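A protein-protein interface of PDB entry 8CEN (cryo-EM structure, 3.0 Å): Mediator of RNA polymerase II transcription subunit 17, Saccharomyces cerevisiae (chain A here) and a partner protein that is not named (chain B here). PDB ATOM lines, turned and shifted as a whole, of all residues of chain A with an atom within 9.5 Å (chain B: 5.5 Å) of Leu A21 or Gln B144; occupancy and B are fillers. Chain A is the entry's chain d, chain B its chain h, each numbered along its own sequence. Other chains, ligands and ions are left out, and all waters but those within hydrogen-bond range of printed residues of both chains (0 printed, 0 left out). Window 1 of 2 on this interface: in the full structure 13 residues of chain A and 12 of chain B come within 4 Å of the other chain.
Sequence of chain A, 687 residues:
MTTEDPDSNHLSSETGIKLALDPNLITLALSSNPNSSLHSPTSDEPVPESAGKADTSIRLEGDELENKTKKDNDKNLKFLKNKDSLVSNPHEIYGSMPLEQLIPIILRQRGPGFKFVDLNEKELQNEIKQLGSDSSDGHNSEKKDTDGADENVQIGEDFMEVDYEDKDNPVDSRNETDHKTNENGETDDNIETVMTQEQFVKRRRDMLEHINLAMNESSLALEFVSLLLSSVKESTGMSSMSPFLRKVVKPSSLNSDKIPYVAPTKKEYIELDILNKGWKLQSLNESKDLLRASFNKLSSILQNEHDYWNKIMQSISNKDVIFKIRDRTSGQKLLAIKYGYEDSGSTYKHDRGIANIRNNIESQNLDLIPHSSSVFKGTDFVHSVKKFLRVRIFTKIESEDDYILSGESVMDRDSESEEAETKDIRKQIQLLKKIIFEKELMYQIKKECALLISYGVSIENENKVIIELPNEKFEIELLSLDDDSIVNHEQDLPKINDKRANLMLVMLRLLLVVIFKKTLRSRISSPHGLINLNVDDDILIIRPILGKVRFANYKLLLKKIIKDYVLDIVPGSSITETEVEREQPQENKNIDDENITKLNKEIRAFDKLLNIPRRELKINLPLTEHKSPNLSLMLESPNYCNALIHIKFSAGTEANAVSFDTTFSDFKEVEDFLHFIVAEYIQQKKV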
ATOM      1  N   ILE A  17      -0.085  23.462  27.070  1.00  0.00           N
ATOM      2  CA  ILE A  17       1.305  23.073  27.268  1.00  0.00           C
ATOM      3  C   ILE A  17       1.509  21.691  26.656  1.00  0.00           C
ATOM      4  O   ILE A  17       0.597  20.860  26.630  1.00  0.00           O
ATOM      5  CB  ILE A  17       1.699  23.117  28.771  1.00  0.00           C
ATOM      6  CG1 ILE A  17       3.213  22.965  28.957  1.00  0.00           C
ATOM      7  CG2 ILE A  17       0.931  22.077  29.584  1.00  0.00           C
ATOM      8  CD1 ILE A  17       3.698  23.316  30.343  1.00  0.00           C
ATOM      9  N   LYS A  18       2.707  21.463  26.123  1.00  0.00           N
ATOM     10  CA  LYS A  18       3.040  20.186  25.515  1.00  0.00           C
ATOM     11  C   LYS A  18       3.172  19.104  26.587  1.00  0.00           C
ATOM     12  O   LYS A  18       3.222  19.380  27.788  1.00  0.00           O
ATOM     13  CB  LYS A  18       4.335  20.300  24.716  1.00  0.00           C
ATOM     14  CG  LYS A  18       4.357  21.446  23.720  1.00  0.00           C
ATOM     15  CD  LYS A  18       5.780  21.774  23.299  1.00  0.00           C
ATOM     16  CE  LYS A  18       5.831  23.014  22.422  1.00  0.00           C
ATOM     17  NZ  LYS A  18       7.232  23.457  22.174  1.00  0.00           N
ATOM     18  N   LEU A  19       3.222  17.852  26.137  1.00  0.00           N
ATOM     19  CA  LEU A  19       3.358  16.710  27.033  1.00  0.00           C
ATOM     20  C   LEU A  19       4.472  15.794  26.556  1.00  0.00           C
ATOM     21  O   LEU A  19       4.514  15.415  25.382  1.00  0.00           O
ATOM     22  CB  LEU A  19       2.049  15.927  27.149  1.00  0.00           C
ATOM     23  CG  LEU A  19       1.100  16.373  28.254  1.00  0.00           C
ATOM     24  CD1 LEU A  19      -0.176  15.553  28.223  1.00  0.00           C
ATOM     25  CD2 LEU A  19       1.806  16.201  29.581  1.00  0.00           C
ATOM     26  N   ALA A  20       5.368  15.441  27.473  1.00  0.00           N
ATOM     27  CA  ALA A  20       6.407  14.449  27.232  1.00  0.00           C
ATOM     28  C   ALA A  20       5.932  13.120  27.800  1.00  0.00           C
ATOM     29  O   ALA A  20       5.624  13.025  28.993  1.00  0.00           O
ATOM     30  CB  ALA A  20       7.730  14.867  27.869  1.00  0.00           C
ATOM     31  N   LEU A  21       5.868  12.101  26.949  1.00  0.00           N
ATOM     32  CA  LEU A  21       5.295  10.818  27.324  1.00  0.00           C
ATOM     33  C   LEU A  21       6.119   9.688  26.732  1.00  0.00           C
ATOM     34  O   LEU A  21       6.805   9.861  25.722  1.00  0.00           O
ATOM     35  CB  LEU A  21       3.838  10.708  26.858  1.00  0.00           C
ATOM     36  CG  LEU A  21       2.794  11.050  27.918  1.00  0.00           C
ATOM     37  CD1 LEU A  21       1.400  10.935  27.362  1.00  0.00           C
ATOM     38  CD2 LEU A  21       2.957  10.101  29.073  1.00  0.00           C
ATOM     39  N   ASP A  22       6.055   8.531  27.384  1.00  0.00           N
ATOM     40  CA  ASP A  22       6.635   7.312  26.842  1.00  0.00           C
ATOM     41  C   ASP A  22       5.543   6.552  26.100  1.00  0.00           C
ATOM     42  O   ASP A  22       4.698   5.906  26.733  1.00  0.00           O
ATOM     43  CB  ASP A  22       7.241   6.453  27.952  1.00  0.00           C
ATOM     44  CG  ASP A  22       8.336   5.533  27.448  1.00  0.00           C
ATOM     45  OD1 ASP A  22       8.382   5.263  26.229  1.00  0.00           O
ATOM     46  OD2 ASP A  22       9.153   5.076  28.274  1.00  0.00           O
ATOM     47  N   PRO A  23       5.525   6.603  24.765  1.00  0.00           N
ATOM     48  CA  PRO A  23       4.422   5.977  24.022  1.00  0.00           C
ATOM     49  C   PRO A  23       4.498   4.462  23.966  1.00  0.00           C
ATOM     50  O   PRO A  23       3.520   3.836  23.540  1.00  0.00           O
ATOM     51  CB  PRO A  23       4.552   6.589  22.624  1.00  0.00           C
ATOM     52  CG  PRO A  23       5.993   6.914  22.492  1.00  0.00           C
ATOM     53  CD  PRO A  23       6.551   7.162  23.869  1.00  0.00           C
ATOM     54  N   ASN A  24       5.616   3.861  24.381  1.00  0.00           N
ATOM     55  CA  ASN A  24       5.747   2.408  24.332  1.00  0.00           C
ATOM     56  C   ASN A  24       4.772   1.717  25.276  1.00  0.00           C
ATOM     57  O   ASN A  24       4.323   0.601  24.993  1.00  0.00           O
ATOM     58  CB  ASN A  24       7.183   2.000  24.664  1.00  0.00           C
ATOM     59  CG  ASN A  24       8.188   2.564  23.682  1.00  0.00           C
ATOM     60  OD1 ASN A  24       7.931   2.621  22.481  1.00  0.00           O
ATOM     61  ND2 ASN A  24       9.338   2.991  24.191  1.00  0.00           N
ATOM     62  N   LEU A  25       4.433   2.355  26.392  1.00  0.00           N
ATOM     63  CA  LEU A  25       3.501   1.792  27.363  1.00  0.00           C
ATOM     64  C   LEU A  25       2.438   2.836  27.681  1.00  0.00           C
ATOM     65  O   LEU A  25       2.759   3.957  28.088  1.00  0.00           O
ATOM     66  CB  LEU A  25       4.250   1.302  28.609  1.00  0.00           C
ATOM     67  CG  LEU A  25       5.094   2.164  29.560  1.00  0.00           C
ATOM     68  CD1 LEU A  25       4.302   2.894  30.646  1.00  0.00           C
ATOM     69  CD2 LEU A  25       6.179   1.306  30.163  1.00  0.00           C
ATOM     70  N   ILE A  26       1.178   2.495  27.412  1.00  0.00           N
ATOM     71  CA  ILE A  26       0.056   3.388  27.676  1.00  0.00           C
ATOM     72  C   ILE A  26      -0.918   2.678  28.608  1.00  0.00           C
ATOM     73  O   ILE A  26      -1.623   3.315  29.399  1.00  0.00           O
ATOM     74  CB  ILE A  26      -0.639   3.817  26.368  1.00  0.00           C
ATOM     75  CG1 ILE A  26       0.390   4.248  25.320  1.00  0.00           C
ATOM     76  CG2 ILE A  26      -1.604   4.962  26.619  1.00  0.00           C
ATOM     77  CD1 ILE A  26       1.123   5.519  25.667  1.00  0.00           C
ATOM     78  N   LEU A  86       3.888   0.424  20.330  1.00  0.00           N
ATOM     79  CA  LEU A  86       3.474   1.129  19.122  1.00  0.00           C
ATOM     80  C   LEU A  86       4.650   1.829  18.450  1.00  0.00           C
ATOM     81  O   LEU A  86       4.685   1.930  17.218  1.00  0.00           O
ATOM     82  CB  LEU A  86       2.338   2.104  19.452  1.00  0.00           C
ATOM     83  CG  LEU A  86       2.501   3.221  20.490  1.00  0.00           C
ATOM     84  CD1 LEU A  86       3.060   4.514  19.913  1.00  0.00           C
ATOM     85  CD2 LEU A  86       1.182   3.478  21.200  1.00  0.00           C
ATOM     86  N   VAL A  87       5.615   2.312  19.225  1.00  0.00           N
ATOM     87  CA  VAL A  87       6.888   2.771  18.682  1.00  0.00           C
ATOM     88  C   VAL A  87       7.851   1.592  18.706  1.00  0.00           C
ATOM     89  O   VAL A  87       8.120   1.019  19.768  1.00  0.00           O
ATOM     90  CB  VAL A  87       7.446   3.963  19.473  1.00  0.00           C
ATOM     91  CG1 VAL A  87       8.902   4.206  19.107  1.00  0.00           C
ATOM     92  CG2 VAL A  87       6.627   5.210  19.198  1.00  0.00           C
ATOM     93  N   ASN B 139      15.022   9.643  23.732  1.00  0.00           N
ATOM     94  CA  ASN B 139      14.795  10.388  22.500  1.00  0.00           C
ATOM     95  C   ASN B 139      13.342  10.295  22.054  1.00  0.00           C
ATOM     96  O   ASN B 139      12.774  11.278  21.571  1.00  0.00           O
ATOM     97  CB  ASN B 139      15.730   9.885  21.401  1.00  0.00           C
ATOM     98  CG  ASN B 139      17.177  10.252  21.655  1.00  0.00           C
ATOM     99  OD1 ASN B 139      17.481  11.367  22.079  1.00  0.00           O
ATOM    100  ND2 ASN B 139      18.081   9.313  21.400  1.00  0.00           N
ATOM    101  N   THR B 140      12.721   9.124  22.220  1.00  0.00           N
ATOM    102  CA  THR B 140      11.307   8.975  21.891  1.00  0.00           C
ATOM    103  C   THR B 140      10.431   9.825  22.807  1.00  0.00           C
ATOM    104  O   THR B 140       9.466  10.456  22.351  1.00  0.00           O
ATOM    105  CB  THR B 140      10.908   7.502  21.976  1.00  0.00           C
ATOM    106  OG1 THR B 140      11.799   6.721  21.171  1.00  0.00           O
ATOM    107  CG2 THR B 140       9.497   7.300  21.465  1.00  0.00           C
ATOM    108  N   ILE B 141      10.765   9.864  24.101  1.00  0.00           N
ATOM    109  CA  ILE B 141      10.018  10.683  25.056  1.00  0.00           C
ATOM    110  C   ILE B 141      10.134  12.163  24.700  1.00  0.00           C
ATOM    111  O   ILE B 141       9.140  12.901  24.713  1.00  0.00           O
ATOM    112  CB  ILE B 141      10.502  10.395  26.491  1.00  0.00           C
ATOM    113  CG1 ILE B 141      10.002   9.024  26.954  1.00  0.00           C
ATOM    114  CG2 ILE B 141      10.047  11.482  27.459  1.00  0.00           C
ATOM    115  CD1 ILE B 141      10.303   8.711  28.405  1.00  0.00           C
ATOM    116  N   LEU B 142      11.341  12.613  24.347  1.00  0.00           N
ATOM    117  CA  LEU B 142      11.522  14.009  23.956  1.00  0.00           C
ATOM    118  C   LEU B 142      10.890  14.314  22.600  1.00  0.00           C
ATOM    119  O   LEU B 142      10.515  15.463  22.342  1.00  0.00           O
ATOM    120  CB  LEU B 142      13.007  14.376  23.945  1.00  0.00           C
ATOM    121  CG  LEU B 142      13.648  14.918  25.232  1.00  0.00           C
ATOM    122  CD1 LEU B 142      13.010  16.247  25.610  1.00  0.00           C
ATOM    123  CD2 LEU B 142      13.584  13.944  26.402  1.00  0.00           C
ATOM    124  N   GLN B 143      10.770  13.318  21.719  1.00  0.00           N
ATOM    125  CA  GLN B 143      10.089  13.538  20.448  1.00  0.00           C
ATOM    126  C   GLN B 143       8.577  13.603  20.615  1.00  0.00           C
ATOM    127  O   GLN B 143       7.900  14.251  19.810  1.00  0.00           O
ATOM    128  CB  GLN B 143      10.459  12.442  19.442  1.00  0.00           C
ATOM    129  CG  GLN B 143      11.837  12.554  18.733  1.00  0.00           C
ATOM    130  CD  GLN B 143      12.037  13.767  17.803  1.00  0.00           C
ATOM    131  OE1 GLN B 143      11.516  14.862  18.019  1.00  0.00           O
ATOM    132  NE2 GLN B 143      12.812  13.549  16.748  1.00  0.00           N
ATOM    133  N   GLN B 144       8.034  12.938  21.638  1.00  0.00           N
ATOM    134  CA  GLN B 144       6.614  13.093  21.949  1.00  0.00           C
ATOM    135  C   GLN B 144       6.267  14.500  22.420  1.00  0.00           C
ATOM    136  O   GLN B 144       5.096  14.889  22.344  1.00  0.00           O
ATOM    137  CB  GLN B 144       6.178  12.083  23.011  1.00  0.00           C
ATOM    138  CG  GLN B 144       6.247  10.637  22.570  1.00  0.00           C
ATOM    139  CD  GLN B 144       5.321  10.339  21.413  1.00  0.00           C
ATOM    140  OE1 GLN B 144       5.764  10.112  20.288  1.00  0.00           O
ATOM    141  NE2 GLN B 144       4.021  10.339  21.685  1.00  0.00           N
ATOM    142  N   ARG B 145       7.253  15.261  22.907  1.00  0.00           N
ATOM    143  CA  ARG B 145       7.008  16.623  23.376  1.00  0.00           C
ATOM    144  C   ARG B 145       6.536  17.532  22.247  1.00  0.00           C
ATOM    145  O   ARG B 145       5.603  18.322  22.425  1.00  0.00           O
ATOM    146  CB  ARG B 145       8.280  17.186  24.012  1.00  0.00           C
ATOM    147  CG  ARG B 145       8.163  18.610  24.528  1.00  0.00           C
ATOM    148  CD  ARG B 145       7.446  18.662  25.865  1.00  0.00           C
ATOM    149  NE  ARG B 145       8.239  18.068  26.934  1.00  0.00           N
ATOM    150  CZ  ARG B 145       9.244  18.673  27.555  1.00  0.00           C
ATOM    151  NH1 ARG B 145       9.602  19.909  27.250  1.00  0.00           N
ATOM    152  NH2 ARG B 145       9.902  18.022  28.508  1.00  0.00           N
ATOM    153  N   SER B 146       7.166  17.429  21.074  1.00  0.00           N
ATOM    154  CA  SER B 146       6.807  18.307  19.966  1.00  0.00           C
ATOM    155  C   SER B 146       5.482  17.908  19.328  1.00  0.00           C
ATOM    156  O   SER B 146       4.763  18.769  18.810  1.00  0.00           O
ATOM    157  CB  SER B 146       7.919  18.310  18.917  1.00  0.00           C
ATOM    158  OG  SER B 146       7.959  17.081  18.215  1.00  0.00           O
ATOM    159  N   LYS B 147       5.141  16.620  19.355  1.00  0.00           N
ATOM    160  CA  LYS B 147       3.936  16.140  18.691  1.00  0.00           C
ATOM    161  C   LYS B 147       2.700  16.160  19.578  1.00  0.00           C
ATOM    162  O   LYS B 147       1.583  16.266  19.060  1.00  0.00           O
ATOM    163  CB  LYS B 147       4.149  14.717  18.166  1.00  0.00           C
ATOM    164  CG  LYS B 147       5.150  14.617  17.030  1.00  0.00           C
ATOM    165  CD  LYS B 147       4.438  14.595  15.685  1.00  0.00           C
ATOM    166  CE  LYS B 147       5.389  14.248  14.553  1.00  0.00           C
ATOM    167  NZ  LYS B 147       4.678  13.599  13.417  1.00  0.00           N
ATOM    168  N   ILE B 148       2.857  16.060  20.894  1.00  0.00           N
ATOM    169  CA  ILE B 148       1.731  15.848  21.795  1.00  0.00           C
ATOM    170  C   ILE B 148       1.461  17.142  22.552  1.00  0.00           C
ATOM    171  O   ILE B 148       2.354  17.684  23.213  1.00  0.00           O
ATOM    172  CB  ILE B 148       2.006  14.685  22.760  1.00  0.00           C
ATOM    173  CG1 ILE B 148       1.892  13.348  22.025  1.00  0.00           C
ATOM    174  CG2 ILE B 148       1.026  14.710  23.914  1.00  0.00           C
ATOM    175  CD1 ILE B 148       0.482  12.905  21.747  1.00  0.00           C
ATOM    176  N   LEU B 153      -4.842  16.924  22.993  1.00  0.00           N
ATOM    177  CA  LEU B 153      -4.992  15.541  23.429  1.00  0.00           C
ATOM    178  C   LEU B 153      -6.333  15.319  24.111  1.00  0.00           C
ATOM    179  O   LEU B 153      -7.062  14.376  23.782  1.00  0.00           O
ATOM    180  CB  LEU B 153      -3.851  15.201  24.385  1.00  0.00           C
ATOM    181  CG  LEU B 153      -3.754  13.855  25.095  1.00  0.00           C
ATOM    182  CD1 LEU B 153      -2.310  13.481  25.119  1.00  0.00           C
ATOM    183  CD2 LEU B 153      -4.288  13.920  26.518  1.00  0.00           C
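O of Ile B148 lies within hydrogen-bond range of N of Leu A19, 3.1 Å away. The backbone carbonyl oxygen (O) of Gln B144 lies close to the backbone carbonyl oxygen (O) of Leu A19 (3.1 Å).
The side-chain carboxylate (OD1) of Asp A22 lies within hydrogen-bond range of the side-chain amide nitrogen (ND2) of Asn A24 (3.2 Å). The side-chain amide oxygen of Asn A24 sits close to the backbone carbonyl oxygen of Val A87 (3.2 Å).
Lys A18 touches Arg B145. Lys A18 touches Ile B148 (CA to O, 3.5 Å). Arg B145 touches Leu A19 (CA to O, 3.4 Å). Ala A20 touches Ile B141 (CB to O, 3.98 Å). NE of Arg B145 touches CB of Ala A20, 3.4 Å away. CG of Gln B144 touches O of Leu A21, 3.3 Å away. Asp A22 touches Ile B141 (CA to CG1, 3.8 Å). CG of Pro A23 touches CG2 of Thr B140, 3.7 Å away. CG of Pro A23 touches CD of Gln B144, 3.7 Å away. Val A87 touches Thr B140 (CG1 to CG2, 3.9 Å).
Printed residues of chain B within 4 Å of Leu A19: Gln B144 (3.1 Å), Arg B145 (3.4 Å) and Ile B148 (3.1 Å). Of chain B, only Ile B141 (3.4 Å) and Gln B144 (3.3 Å) come within 4 Å of Leu A21. Printed residues of chain B within 4 Å of Asp A22: Ile B141 (3.8 Å). Ile B141 touches three residues of chain A. Gln B144 touches just these residues of chain A: Leu A19, Leu A21 and Pro A23. No residue of chain A comes within 4 Å of Ser B146. The nearest printed residue of chain B that does not touch Val A87 is Gln B144 (5.1 Å).
Of the 11 printed residues of chain B, 5 touch a printed residue of chain A. Hydrophobic or aromatic side chains of chain B within 4 Å of the printed part of chain A: Ile B141 and Ile B148. Of the 12 printed residues of chain A, 7 touch a printed residue of chain B. Among the printed residues, 13 pairs touch across the chains.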
